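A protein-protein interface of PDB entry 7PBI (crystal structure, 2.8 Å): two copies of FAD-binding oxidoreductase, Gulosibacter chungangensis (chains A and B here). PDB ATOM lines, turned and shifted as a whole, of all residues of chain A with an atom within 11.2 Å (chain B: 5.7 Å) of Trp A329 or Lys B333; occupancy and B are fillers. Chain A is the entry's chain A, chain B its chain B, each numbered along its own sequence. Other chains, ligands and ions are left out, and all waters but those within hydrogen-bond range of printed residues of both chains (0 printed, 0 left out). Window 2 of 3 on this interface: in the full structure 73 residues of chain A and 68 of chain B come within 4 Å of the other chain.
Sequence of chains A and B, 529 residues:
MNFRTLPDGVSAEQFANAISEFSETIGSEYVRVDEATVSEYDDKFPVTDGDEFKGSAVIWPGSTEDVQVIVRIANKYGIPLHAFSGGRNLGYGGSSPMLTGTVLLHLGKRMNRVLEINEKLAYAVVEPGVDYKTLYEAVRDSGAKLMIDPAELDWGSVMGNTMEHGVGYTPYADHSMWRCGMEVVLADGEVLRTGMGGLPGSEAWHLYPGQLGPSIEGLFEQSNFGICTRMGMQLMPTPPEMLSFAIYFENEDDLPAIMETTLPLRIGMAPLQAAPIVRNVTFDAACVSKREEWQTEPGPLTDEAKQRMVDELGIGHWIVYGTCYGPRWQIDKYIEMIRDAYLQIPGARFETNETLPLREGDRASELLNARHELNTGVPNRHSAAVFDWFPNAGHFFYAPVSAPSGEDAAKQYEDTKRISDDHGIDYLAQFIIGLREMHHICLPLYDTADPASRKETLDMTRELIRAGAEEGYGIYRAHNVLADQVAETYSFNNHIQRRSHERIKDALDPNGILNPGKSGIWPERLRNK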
ATOM      1  N   PRO A 239      -2.890 -12.939  33.516  1.00  0.00           N
ATOM      2  CA  PRO A 239      -2.117 -12.055  32.643  1.00  0.00           C
ATOM      3  C   PRO A 239      -0.762 -11.756  33.280  1.00  0.00           C
ATOM      4  O   PRO A 239      -0.518 -12.129  34.429  1.00  0.00           O
ATOM      5  CB  PRO A 239      -2.997 -10.799  32.544  1.00  0.00           C
ATOM      6  CG  PRO A 239      -3.757 -10.773  33.864  1.00  0.00           C
ATOM      7  CD  PRO A 239      -3.916 -12.221  34.287  1.00  0.00           C
ATOM      8  N   PRO A 240       0.156 -11.064  32.566  1.00  0.00           N
ATOM      9  CA  PRO A 240       1.469 -10.737  33.120  1.00  0.00           C
ATOM     10  C   PRO A 240       1.405  -9.750  34.289  1.00  0.00           C
ATOM     11  O   PRO A 240       2.166  -9.905  35.197  1.00  0.00           O
ATOM     12  CB  PRO A 240       2.222 -10.084  31.957  1.00  0.00           C
ATOM     13  CG  PRO A 240       1.451 -10.510  30.728  1.00  0.00           C
ATOM     14  CD  PRO A 240       0.008 -10.584  31.185  1.00  0.00           C
ATOM     15  N   GLU A 241       0.518  -8.760  34.231  1.00  0.00           N
ATOM     16  CA  GLU A 241       0.409  -7.722  35.289  1.00  0.00           C
ATOM     17  C   GLU A 241      -1.044  -7.331  35.491  1.00  0.00           C
ATOM     18  O   GLU A 241      -1.833  -7.489  34.568  1.00  0.00           O
ATOM     19  CB  GLU A 241       1.146  -6.433  34.921  1.00  0.00           C
ATOM     20  CG  GLU A 241       2.614  -6.630  34.636  1.00  0.00           C
ATOM     21  CD  GLU A 241       3.366  -7.098  35.861  1.00  0.00           C
ATOM     22  OE1 GLU A 241       4.562  -7.376  35.739  1.00  0.00           O
ATOM     23  OE2 GLU A 241       2.738  -7.187  36.934  1.00  0.00           O
ATOM     24  N   MET A 242      -1.339  -6.760  36.649  1.00  0.00           N
ATOM     25  CA  MET A 242      -2.681  -6.244  36.970  1.00  0.00           C
ATOM     26  C   MET A 242      -2.540  -5.003  37.845  1.00  0.00           C
ATOM     27  O   MET A 242      -1.716  -5.004  38.766  1.00  0.00           O
ATOM     28  CB  MET A 242      -3.474  -7.329  37.687  1.00  0.00           C
ATOM     29  CG  MET A 242      -3.745  -8.486  36.776  1.00  0.00           C
ATOM     30  SD  MET A 242      -4.808  -9.704  37.528  1.00  0.00           S
ATOM     31  CE  MET A 242      -3.601 -10.656  38.445  1.00  0.00           C
ATOM     32  N   LEU A 243      -3.300  -3.963  37.538  1.00  0.00           N
ATOM     33  CA  LEU A 243      -3.224  -2.710  38.313  1.00  0.00           C
ATOM     34  C   LEU A 243      -4.628  -2.213  38.625  1.00  0.00           C
ATOM     35  O   LEU A 243      -5.420  -2.056  37.695  1.00  0.00           O
ATOM     36  CB  LEU A 243      -2.433  -1.671  37.521  1.00  0.00           C
ATOM     37  CG  LEU A 243      -1.821  -0.573  38.389  1.00  0.00           C
ATOM     38  CD1 LEU A 243      -0.811  -1.156  39.364  1.00  0.00           C
ATOM     39  CD2 LEU A 243      -1.177   0.493  37.524  1.00  0.00           C
ATOM     40  N   ALA A 270     -12.564  -2.056  26.401  1.00  0.00           N
ATOM     41  CA  ALA A 270     -11.266  -1.372  26.567  1.00  0.00           C
ATOM     42  C   ALA A 270     -11.512   0.132  26.533  1.00  0.00           C
ATOM     43  O   ALA A 270     -12.372   0.587  25.792  1.00  0.00           O
ATOM     44  CB  ALA A 270     -10.317  -1.814  25.484  1.00  0.00           C
ATOM     45  N   PRO A 271     -10.823   0.965  27.343  1.00  0.00           N
ATOM     46  CA  PRO A 271      -9.802   0.519  28.295  1.00  0.00           C
ATOM     47  C   PRO A 271     -10.309  -0.123  29.601  1.00  0.00           C
ATOM     48  O   PRO A 271      -9.476  -0.587  30.382  1.00  0.00           O
ATOM     49  CB  PRO A 271      -9.073   1.834  28.629  1.00  0.00           C
ATOM     50  CG  PRO A 271     -10.153   2.883  28.520  1.00  0.00           C
ATOM     51  CD  PRO A 271     -11.002   2.422  27.354  1.00  0.00           C
ATOM     52  N   GLN A 273     -11.446  -3.116  30.945  1.00  0.00           N
ATOM     53  CA  GLN A 273     -11.446  -4.560  30.583  1.00  0.00           C
ATOM     54  C   GLN A 273     -12.357  -5.348  31.529  1.00  0.00           C
ATOM     55  O   GLN A 273     -12.569  -6.532  31.288  1.00  0.00           O
ATOM     56  CB  GLN A 273     -10.028  -5.123  30.649  1.00  0.00           C
ATOM     57  CG  GLN A 273      -9.046  -4.418  29.719  1.00  0.00           C
ATOM     58  CD  GLN A 273      -7.637  -4.533  30.241  1.00  0.00           C
ATOM     59  OE1 GLN A 273      -7.209  -3.765  31.098  1.00  0.00           O
ATOM     60  NE2 GLN A 273      -6.908  -5.519  29.750  1.00  0.00           N
ATOM     61  N   CYS A 324      -6.978  -2.834  35.434  1.00  0.00           N
ATOM     62  CA  CYS A 324      -6.462  -3.135  34.080  1.00  0.00           C
ATOM     63  C   CYS A 324      -5.517  -4.334  34.136  1.00  0.00           C
ATOM     64  O   CYS A 324      -4.864  -4.562  35.169  1.00  0.00           O
ATOM     65  CB  CYS A 324      -5.797  -1.912  33.482  1.00  0.00           C
ATOM     66  SG  CYS A 324      -6.936  -0.511  33.511  1.00  0.00           S
ATOM     67  N   TYR A 325      -5.494  -5.073  33.037  1.00  0.00           N
ATOM     68  CA  TYR A 325      -4.877  -6.410  32.914  1.00  0.00           C
ATOM     69  C   TYR A 325      -4.009  -6.415  31.665  1.00  0.00           C
ATOM     70  O   TYR A 325      -4.411  -5.798  30.665  1.00  0.00           O
ATOM     71  CB  TYR A 325      -5.960  -7.483  32.790  1.00  0.00           C
ATOM     72  CG  TYR A 325      -6.967  -7.476  33.908  1.00  0.00           C
ATOM     73  CD1 TYR A 325      -8.044  -6.610  33.898  1.00  0.00           C
ATOM     74  CD2 TYR A 325      -6.841  -8.342  34.979  1.00  0.00           C
ATOM     75  CE1 TYR A 325      -8.969  -6.601  34.926  1.00  0.00           C
ATOM     76  CE2 TYR A 325      -7.762  -8.352  36.012  1.00  0.00           C
ATOM     77  CZ  TYR A 325      -8.829  -7.477  35.982  1.00  0.00           C
ATOM     78  OH  TYR A 325      -9.742  -7.465  36.994  1.00  0.00           O
ATOM     79  N   GLY A 326      -2.889  -7.125  31.726  1.00  0.00           N
ATOM     80  CA  GLY A 326      -1.980  -7.330  30.590  1.00  0.00           C
ATOM     81  C   GLY A 326      -0.581  -6.825  30.920  1.00  0.00           C
ATOM     82  O   GLY A 326      -0.251  -6.553  32.076  1.00  0.00           O
ATOM     83  N   PRO A 327       0.230  -6.667  29.828  1.00  0.00           N
ATOM     84  CA  PRO A 327       1.541  -6.176  30.134  1.00  0.00           C
ATOM     85  C   PRO A 327       1.474  -4.710  30.359  1.00  0.00           C
ATOM     86  O   PRO A 327       0.473  -4.075  30.073  1.00  0.00           O
ATOM     87  CB  PRO A 327       2.312  -6.477  28.857  1.00  0.00           C
ATOM     88  CG  PRO A 327       1.503  -7.441  28.084  1.00  0.00           C
ATOM     89  CD  PRO A 327       0.155  -6.921  28.362  1.00  0.00           C
ATOM     90  N   ARG A 328       2.556  -4.147  30.833  1.00  0.00           N
ATOM     91  CA  ARG A 328       2.537  -2.758  31.170  1.00  0.00           C
ATOM     92  C   ARG A 328       2.171  -1.845  30.037  1.00  0.00           C
ATOM     93  O   ARG A 328       1.470  -0.894  30.262  1.00  0.00           O
ATOM     94  CB  ARG A 328       3.876  -2.355  31.760  1.00  0.00           C
ATOM     95  CG  ARG A 328       3.785  -1.673  33.105  1.00  0.00           C
ATOM     96  CD  ARG A 328       4.995  -0.785  33.309  1.00  0.00           C
ATOM     97  NE  ARG A 328       5.963  -1.389  34.217  1.00  0.00           N
ATOM     98  CZ  ARG A 328       6.670  -0.704  35.107  1.00  0.00           C
ATOM     99  NH1 ARG A 328       7.529  -1.329  35.899  1.00  0.00           N
ATOM    100  NH2 ARG A 328       6.514   0.608  35.203  1.00  0.00           N
ATOM    101  N   TRP A 329       2.636  -2.108  28.831  1.00  0.00           N
ATOM    102  CA  TRP A 329       2.374  -1.181  27.752  1.00  0.00           C
ATOM    103  C   TRP A 329       0.894  -0.950  27.658  1.00  0.00           C
ATOM    104  O   TRP A 329       0.465   0.170  27.563  1.00  0.00           O
ATOM    105  CB  TRP A 329       2.967  -1.677  26.422  1.00  0.00           C
ATOM    106  CG  TRP A 329       2.754  -3.098  26.016  1.00  0.00           C
ATOM    107  CD1 TRP A 329       3.555  -4.151  26.303  1.00  0.00           C
ATOM    108  CD2 TRP A 329       1.711  -3.604  25.178  1.00  0.00           C
ATOM    109  NE1 TRP A 329       3.063  -5.290  25.728  1.00  0.00           N
ATOM    110  CE2 TRP A 329       1.925  -4.981  25.036  1.00  0.00           C
ATOM    111  CE3 TRP A 329       0.605  -3.030  24.552  1.00  0.00           C
ATOM    112  CZ2 TRP A 329       1.075  -5.791  24.299  1.00  0.00           C
ATOM    113  CZ3 TRP A 329      -0.236  -3.834  23.826  1.00  0.00           C
ATOM    114  CH2 TRP A 329       0.002  -5.197  23.702  1.00  0.00           C
ATOM    115  N   GLN A 330       0.121  -1.998  27.731  1.00  0.00           N
ATOM    116  CA  GLN A 330      -1.360  -1.976  27.659  1.00  0.00           C
ATOM    117  C   GLN A 330      -1.913  -1.267  28.902  1.00  0.00           C
ATOM    118  O   GLN A 330      -2.767  -0.352  28.753  1.00  0.00           O
ATOM    119  CB  GLN A 330      -1.899  -3.402  27.530  1.00  0.00           C
ATOM    120  CG  GLN A 330      -3.328  -3.449  27.023  1.00  0.00           C
ATOM    121  CD  GLN A 330      -3.715  -4.825  26.550  1.00  0.00           C
ATOM    122  OE1 GLN A 330      -3.297  -5.839  27.109  1.00  0.00           O
ATOM    123  NE2 GLN A 330      -4.533  -4.854  25.512  1.00  0.00           N
ATOM    124  N   ILE A 331      -1.437  -1.659  30.087  1.00  0.00           N
ATOM    125  CA  ILE A 331      -1.935  -1.118  31.384  1.00  0.00           C
ATOM    126  C   ILE A 331      -1.717   0.395  31.423  1.00  0.00           C
ATOM    127  O   ILE A 331      -2.694   1.101  31.701  1.00  0.00           O
ATOM    128  CB  ILE A 331      -1.289  -1.831  32.578  1.00  0.00           C
ATOM    129  CG1 ILE A 331      -1.623  -3.327  32.555  1.00  0.00           C
ATOM    130  CG2 ILE A 331      -1.734  -1.150  33.858  1.00  0.00           C
ATOM    131  CD1 ILE A 331      -1.369  -4.080  33.844  1.00  0.00           C
ATOM    132  N   ASP A 332      -0.507   0.864  31.111  1.00  0.00           N
ATOM    133  CA  ASP A 332      -0.150   2.308  31.076  1.00  0.00           C
ATOM    134  C   ASP A 332      -1.053   3.055  30.096  1.00  0.00           C
ATOM    135  O   ASP A 332      -1.573   4.119  30.464  1.00  0.00           O
ATOM    136  CB  ASP A 332       1.302   2.528  30.665  1.00  0.00           C
ATOM    137  CG  ASP A 332       2.297   1.785  31.536  1.00  0.00           C
ATOM    138  OD1 ASP A 332       1.924   1.386  32.663  1.00  0.00           O
ATOM    139  OD2 ASP A 332       3.437   1.608  31.073  1.00  0.00           O
ATOM    140  N   LYS A 333      -1.228   2.535  28.886  1.00  0.00           N
ATOM    141  CA  LYS A 333      -2.118   3.184  27.890  1.00  0.00           C
ATOM    142  C   LYS A 333      -3.530   3.187  28.489  1.00  0.00           C
ATOM    143  O   LYS A 333      -4.133   4.265  28.549  1.00  0.00           O
ATOM    144  CB  LYS A 333      -2.037   2.504  26.517  1.00  0.00           C
ATOM    145  CG  LYS A 333      -0.647   2.439  25.887  1.00  0.00           C
ATOM    146  CD  LYS A 333      -0.106   3.771  25.430  1.00  0.00           C
ATOM    147  CE  LYS A 333      -0.819   4.282  24.199  1.00  0.00           C
ATOM    148  NZ  LYS A 333      -0.171   5.496  23.652  1.00  0.00           N
ATOM    149  N   TYR A 334      -4.016   2.042  28.975  1.00  0.00           N
ATOM    150  CA  TYR A 334      -5.398   1.919  29.500  1.00  0.00           C
ATOM    151  C   TYR A 334      -5.547   2.825  30.720  1.00  0.00           C
ATOM    152  O   TYR A 334      -6.513   3.619  30.761  1.00  0.00           O
ATOM    153  CB  TYR A 334      -5.767   0.463  29.794  1.00  0.00           C
ATOM    154  CG  TYR A 334      -6.082  -0.373  28.575  1.00  0.00           C
ATOM    155  CD1 TYR A 334      -6.187   0.193  27.312  1.00  0.00           C
ATOM    156  CD2 TYR A 334      -6.292  -1.740  28.686  1.00  0.00           C
ATOM    157  CE1 TYR A 334      -6.463  -0.573  26.194  1.00  0.00           C
ATOM    158  CE2 TYR A 334      -6.580  -2.520  27.577  1.00  0.00           C
ATOM    159  CZ  TYR A 334      -6.663  -1.934  26.326  1.00  0.00           C
ATOM    160  OH  TYR A 334      -6.938  -2.671  25.208  1.00  0.00           O
ATOM    161  N   ILE A 335      -4.623   2.729  31.674  1.00  0.00           N
ATOM    162  CA  ILE A 335      -4.675   3.563  32.911  1.00  0.00           C
ATOM    163  C   ILE A 335      -4.645   5.045  32.512  1.00  0.00           C
ATOM    164  O   ILE A 335      -5.366   5.838  33.130  1.00  0.00           O
ATOM    165  CB  ILE A 335      -3.561   3.205  33.916  1.00  0.00           C
ATOM    166  CG1 ILE A 335      -3.806   1.835  34.563  1.00  0.00           C
ATOM    167  CG2 ILE A 335      -3.420   4.298  34.963  1.00  0.00           C
ATOM    168  CD1 ILE A 335      -4.971   1.795  35.543  1.00  0.00           C
ATOM    169  N   GLU A 336      -3.872   5.419  31.500  1.00  0.00           N
ATOM    170  CA  GLU A 336      -3.780   6.847  31.108  1.00  0.00           C
ATOM    171  C   GLU A 336      -5.126   7.358  30.572  1.00  0.00           C
ATOM    172  O   GLU A 336      -5.483   8.504  30.894  1.00  0.00           O
ATOM    173  CB  GLU A 336      -2.672   7.078  30.084  1.00  0.00           C
ATOM    174  CG  GLU A 336      -1.940   8.374  30.354  1.00  0.00           C
ATOM    175  CD  GLU A 336      -1.446   8.486  31.795  1.00  0.00           C
ATOM    176  OE1 GLU A 336      -0.653   7.609  32.230  1.00  0.00           O
ATOM    177  OE2 GLU A 336      -1.880   9.425  32.499  1.00  0.00           O
ATOM    178  N   MET A 337      -5.832   6.553  29.774  1.00  0.00           N
ATOM    179  CA  MET A 337      -7.132   6.920  29.156  1.00  0.00           C
ATOM    180  C   MET A 337      -8.212   6.998  30.245  1.00  0.00           C
ATOM    181  O   MET A 337      -9.037   7.943  30.209  1.00  0.00           O
ATOM    182  CB  MET A 337      -7.545   5.880  28.108  1.00  0.00           C
ATOM    183  CG  MET A 337      -6.505   5.665  27.013  1.00  0.00           C
ATOM    184  SD  MET A 337      -7.002   4.445  25.761  1.00  0.00           S
ATOM    185  CE  MET A 337      -8.452   5.264  25.089  1.00  0.00           C
ATOM    186  N   ILE A 338      -8.227   6.032  31.171  1.00  0.00           N
ATOM    187  CA  ILE A 338      -9.195   6.013  32.303  1.00  0.00           C
ATOM    188  C   ILE A 338      -8.977   7.290  33.133  1.00  0.00           C
ATOM    189  O   ILE A 338      -9.960   8.037  33.312  1.00  0.00           O
ATOM    190  CB  ILE A 338      -9.061   4.706  33.114  1.00  0.00           C
ATOM    191  CG1 ILE A 338      -9.502   3.508  32.268  1.00  0.00           C
ATOM    192  CG2 ILE A 338      -9.827   4.781  34.433  1.00  0.00           C
ATOM    193  CD1 ILE A 338      -8.941   2.165  32.714  1.00  0.00           C
ATOM    194  N   ARG B 328      -3.111   1.453  16.684  1.00  0.00           N
ATOM    195  CA  ARG B 328      -1.967   0.979  15.873  1.00  0.00           C
ATOM    196  C   ARG B 328      -0.869   0.429  16.787  1.00  0.00           C
ATOM    197  O   ARG B 328      -0.206  -0.526  16.369  1.00  0.00           O
ATOM    198  CB  ARG B 328      -1.419   2.078  14.961  1.00  0.00           C
ATOM    199  CG  ARG B 328      -0.569   1.534  13.821  1.00  0.00           C
ATOM    200  CD  ARG B 328      -1.332   0.537  12.955  1.00  0.00           C
ATOM    201  NE  ARG B 328      -0.493  -0.478  12.320  1.00  0.00           N
ATOM    202  CZ  ARG B 328      -0.211  -0.531  11.018  1.00  0.00           C
ATOM    203  NH1 ARG B 328      -0.686   0.388  10.191  1.00  0.00           N
ATOM    204  NH2 ARG B 328       0.556  -1.499  10.544  1.00  0.00           N
ATOM    205  N   TRP B 329      -0.690   0.991  17.984  1.00  0.00           N
ATOM    206  CA  TRP B 329       0.337   0.521  18.960  1.00  0.00           C
ATOM    207  C   TRP B 329       0.001  -0.887  19.492  1.00  0.00           C
ATOM    208  O   TRP B 329       0.953  -1.618  19.869  1.00  0.00           O
ATOM    209  CB  TRP B 329       0.541   1.527  20.107  1.00  0.00           C
ATOM    210  CG  TRP B 329      -0.684   1.877  20.895  1.00  0.00           C
ATOM    211  CD1 TRP B 329      -1.453   2.992  20.743  1.00  0.00           C
ATOM    212  CD2 TRP B 329      -1.271   1.123  21.971  1.00  0.00           C
ATOM    213  NE1 TRP B 329      -2.491   2.975  21.635  1.00  0.00           N
ATOM    214  CE2 TRP B 329      -2.407   1.841  22.403  1.00  0.00           C
ATOM    215  CE3 TRP B 329      -0.980  -0.101  22.585  1.00  0.00           C
ATOM    216  CZ2 TRP B 329      -3.232   1.388  23.434  1.00  0.00           C
ATOM    217  CZ3 TRP B 329      -1.793  -0.543  23.607  1.00  0.00           C
ATOM    218  CH2 TRP B 329      -2.899   0.193  24.024  1.00  0.00           C
ATOM    219  N   GLN B 330      -1.287  -1.246  19.549  1.00  0.00           N
ATOM    220  CA  GLN B 330      -1.757  -2.574  20.031  1.00  0.00           C
ATOM    221  C   GLN B 330      -1.576  -3.596  18.900  1.00  0.00           C
ATOM    222  O   GLN B 330      -0.944  -4.653  19.118  1.00  0.00           O
ATOM    223  CB  GLN B 330      -3.207  -2.488  20.522  1.00  0.00           C
ATOM    224  CG  GLN B 330      -3.651  -3.735  21.277  1.00  0.00           C
ATOM    225  CD  GLN B 330      -4.993  -3.629  21.960  1.00  0.00           C
ATOM    226  OE1 GLN B 330      -5.562  -2.555  22.148  1.00  0.00           O
ATOM    227  NE2 GLN B 330      -5.509  -4.771  22.372  1.00  0.00           N
ATOM    228  N   ILE B 331      -2.072  -3.270  17.714  1.00  0.00           N
ATOM    229  CA  ILE B 331      -2.003  -4.167  16.524  1.00  0.00           C
ATOM    230  C   ILE B 331      -0.536  -4.547  16.275  1.00  0.00           C
ATOM    231  O   ILE B 331      -0.281  -5.723  15.946  1.00  0.00           O
ATOM    232  CB  ILE B 331      -2.667  -3.528  15.281  1.00  0.00           C
ATOM    233  CG1 ILE B 331      -4.159  -3.253  15.504  1.00  0.00           C
ATOM    234  CG2 ILE B 331      -2.453  -4.410  14.061  1.00  0.00           C
ATOM    235  CD1 ILE B 331      -4.787  -2.380  14.458  1.00  0.00           C
ATOM    236  N   ASP B 332       0.396  -3.603  16.445  1.00  0.00           N
ATOM    237  CA  ASP B 332       1.832  -3.801  16.101  1.00  0.00           C
ATOM    238  C   ASP B 332       2.437  -4.831  17.066  1.00  0.00           C
ATOM    239  O   ASP B 332       3.182  -5.733  16.609  1.00  0.00           O
ATOM    240  CB  ASP B 332       2.610  -2.477  16.095  1.00  0.00           C
ATOM    241  CG  ASP B 332       2.264  -1.500  14.973  1.00  0.00           C
ATOM    242  OD1 ASP B 332       1.677  -1.915  13.954  1.00  0.00           O
ATOM    243  OD2 ASP B 332       2.584  -0.312  15.136  1.00  0.00           O
ATOM    244  N   LYS B 333       2.108  -4.729  18.352  1.00  0.00           N
ATOM    245  CA  LYS B 333       2.592  -5.691  19.370  1.00  0.00           C
ATOM    246  C   LYS B 333       1.994  -7.064  19.052  1.00  0.00           C
ATOM    247  O   LYS B 333       2.770  -8.030  19.007  1.00  0.00           O
ATOM    248  CB  LYS B 333       2.259  -5.212  20.785  1.00  0.00           C
ATOM    249  CG  LYS B 333       2.901  -3.886  21.204  1.00  0.00           C
ATOM    250  CD  LYS B 333       4.421  -3.859  21.146  1.00  0.00           C
ATOM    251  CE  LYS B 333       5.100  -4.883  22.039  1.00  0.00           C
ATOM    252  NZ  LYS B 333       5.601  -4.279  23.294  1.00  0.00           N
ATOM    253  N   TYR B 334       0.683  -7.153  18.800  1.00  0.00           N
ATOM    254  CA  TYR B 334      -0.020  -8.459  18.655  1.00  0.00           C
ATOM    255  C   TYR B 334       0.460  -9.175  17.395  1.00  0.00           C
ATOM    256  O   TYR B 334       0.783 -10.390  17.480  1.00  0.00           O
ATOM    257  CB  TYR B 334      -1.545  -8.313  18.637  1.00  0.00           C
ATOM    258  CG  TYR B 334      -2.157  -7.974  19.974  1.00  0.00           C
ATOM    259  CD1 TYR B 334      -1.464  -8.173  21.155  1.00  0.00           C
ATOM    260  CD2 TYR B 334      -3.437  -7.460  20.058  1.00  0.00           C
ATOM    261  CE1 TYR B 334      -2.016  -7.850  22.380  1.00  0.00           C
ATOM    262  CE2 TYR B 334      -4.006  -7.139  21.277  1.00  0.00           C
ATOM    263  CZ  TYR B 334      -3.291  -7.331  22.443  1.00  0.00           C
ATOM    264  OH  TYR B 334      -3.831  -7.026  23.657  1.00  0.00           O
ATOM    265  N   ILE B 335       0.498  -8.448  16.275  1.00  0.00           N
ATOM    266  CA  ILE B 335       0.898  -8.987  14.942  1.00  0.00           C
ATOM    267  C   ILE B 335       2.257  -9.673  15.074  1.00  0.00           C
ATOM    268  O   ILE B 335       2.510 -10.663  14.346  1.00  0.00           O
ATOM    269  CB  ILE B 335       0.937  -7.873  13.874  1.00  0.00           C
ATOM    270  CG1 ILE B 335      -0.468  -7.560  13.343  1.00  0.00           C
ATOM    271  CG2 ILE B 335       1.901  -8.218  12.745  1.00  0.00           C
ATOM    272  CD1 ILE B 335      -1.195  -8.749  12.723  1.00  0.00           C
ATOM    273  N   GLU B 336       3.118  -9.148  15.944  1.00  0.00           N
ATOM    274  CA  GLU B 336       4.512  -9.627  15.998  1.00  0.00           C
ATOM    275  C   GLU B 336       4.637 -10.839  16.914  1.00  0.00           C
ATOM    276  O   GLU B 336       5.507 -11.675  16.633  1.00  0.00           O
ATOM    277  CB  GLU B 336       5.472  -8.533  16.428  1.00  0.00           C
ATOM    278  CG  GLU B 336       6.870  -8.849  15.940  1.00  0.00           C
ATOM    279  CD  GLU B 336       7.534  -7.753  15.118  1.00  0.00           C
ATOM    280  OE1 GLU B 336       6.895  -6.694  14.902  1.00  0.00           O
ATOM    281  OE2 GLU B 336       8.692  -7.963  14.687  1.00  0.00           O
ATOM    282  N   MET B 337       3.835 -10.932  17.972  1.00  0.00           N
ATOM    283  CA  MET B 337       3.753 -12.186  18.757  1.00  0.00           C
ATOM    284  C   MET B 337       3.274 -13.300  17.831  1.00  0.00           C
ATOM    285  O   MET B 337       3.918 -14.379  17.816  1.00  0.00           O
ATOM    286  CB  MET B 337       2.787 -12.060  19.930  1.00  0.00           C
ATOM    287  CG  MET B 337       3.427 -11.464  21.132  1.00  0.00           C
ATOM    288  SD  MET B 337       2.176 -11.075  22.340  1.00  0.00           S
ATOM    289  CE  MET B 337       1.969  -9.328  22.003  1.00  0.00           C
ATOM    290  N   ILE B 338       2.200 -13.029  17.081  1.00  0.00           N
ATOM    291  CA  ILE B 338       1.579 -14.015  16.154  1.00  0.00           C
ATOM    292  C   ILE B 338       2.647 -14.441  15.137  1.00  0.00           C
ATOM    293  O   ILE B 338       2.900 -15.653  15.026  1.00  0.00           O
ATOM    294  CB  ILE B 338       0.309 -13.432  15.505  1.00  0.00           C
ATOM    295  CG1 ILE B 338      -0.731 -13.075  16.567  1.00  0.00           C
ATOM    296  CG2 ILE B 338      -0.257 -14.390  14.467  1.00  0.00           C
ATOM    297  CD1 ILE B 338      -1.743 -12.053  16.116  1.00  0.00           C
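Of the 23 printed residues of chain A, 4 touch a printed residue of chain B.
Hydrophobic or aromatic side chains of chain A that line the printed part of chain B: Trp A329 and Tyr A334.
Of the 11 printed residues of chain B, 4 touch a printed residue of chain A.
Hydrophobic or aromatic side chains of chain B that line the printed part of chain A: Trp B329 and Tyr B334.
Among the printed residues, 7 pairs touch across the chains.
The side-chain amide nitrogen of Gln A330 sits close to the side-chain amide nitrogen of Gln B330 (3.3 Å).
The side-chain amide nitrogen (NE2) of Gln A330 sits at hydrogen-bond distance from the side-chain hydroxyl (OH) of Tyr B334 (2.9 Å).
The side-chain hydroxyl of Tyr A334 sits at hydrogen-bond distance from the side-chain amide oxygen of Gln B330, at 3.4 Å.
Trp A329 touches its own counterpart, Trp B329.
Trp A329 touches Lys B333, and with the chains exchanged Lys A333 touches Trp B329.
Gln B330 touches its own counterpart, Gln A330.
Gln A330 touches Tyr B334, and with the chains exchanged Tyr A334 touches Gln B330.
Positions printed for both chains: 328, 329, 330, 331, 332, 333, 334, 335, 336, 337 and 338.
Of the 7 pairs that touch across the chains among the printed residues, 6 have their exchanged pair printed and touching as well.
Among the printed residues, pairs that only touch across the chains: Lys A333 with Trp B329 (3.3 Å), Trp A329 with Trp B329 (3.6 Å), Trp A329 with Tyr B334 (3.6 Å) and Trp A329 with Lys B333 (3.6 Å).
The side-chain amide nitrogen (NE2) of Gln A330 sits at hydrogen-bond distance from the side-chain hydroxyl (OH) of Tyr A334, 3.3 Å away.
The side-chain amide nitrogen of Gln B330 lies close to the side-chain hydroxyl of Tyr B334.
Cys A324 touches none of the printed residues of chain B.
Trp A329 touches just these residues of chain B: Trp B329 (3.6 Å), Lys B333 (3.6 Å) and Tyr B334 (3.6 Å).
Of the printed residues of chain B, Gln A330 touches Gln B330 (3.3 Å) and Tyr B334 (2.9 Å).
Printed residues of chain B within 4 Å of Lys A333: Trp B329.
Of the printed residues of chain B, Tyr A334 touches Gln B330 (3.4 Å).
Printed residues of chain A within 4 Å of Trp B329: Trp A329 (3.6 Å) and Lys A333 (3.3 Å).
Of chain A, only Gln A330 (3.3 Å) and Tyr A334 (3.4 Å) come within 4 Å of Gln B330.
No residue of chain A comes within 4 Å of Asp B332.
Lys B333 touches one residue of chain A.
No residue of chain A comes within 4 Å of Met B337.
The nearest residue of chain B that does not touch Trp A329 is Gln B330 (4.3 Å).
The nearest residue of chain A that does not touch Lys B333 is Pro A327 (6.8 Å).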
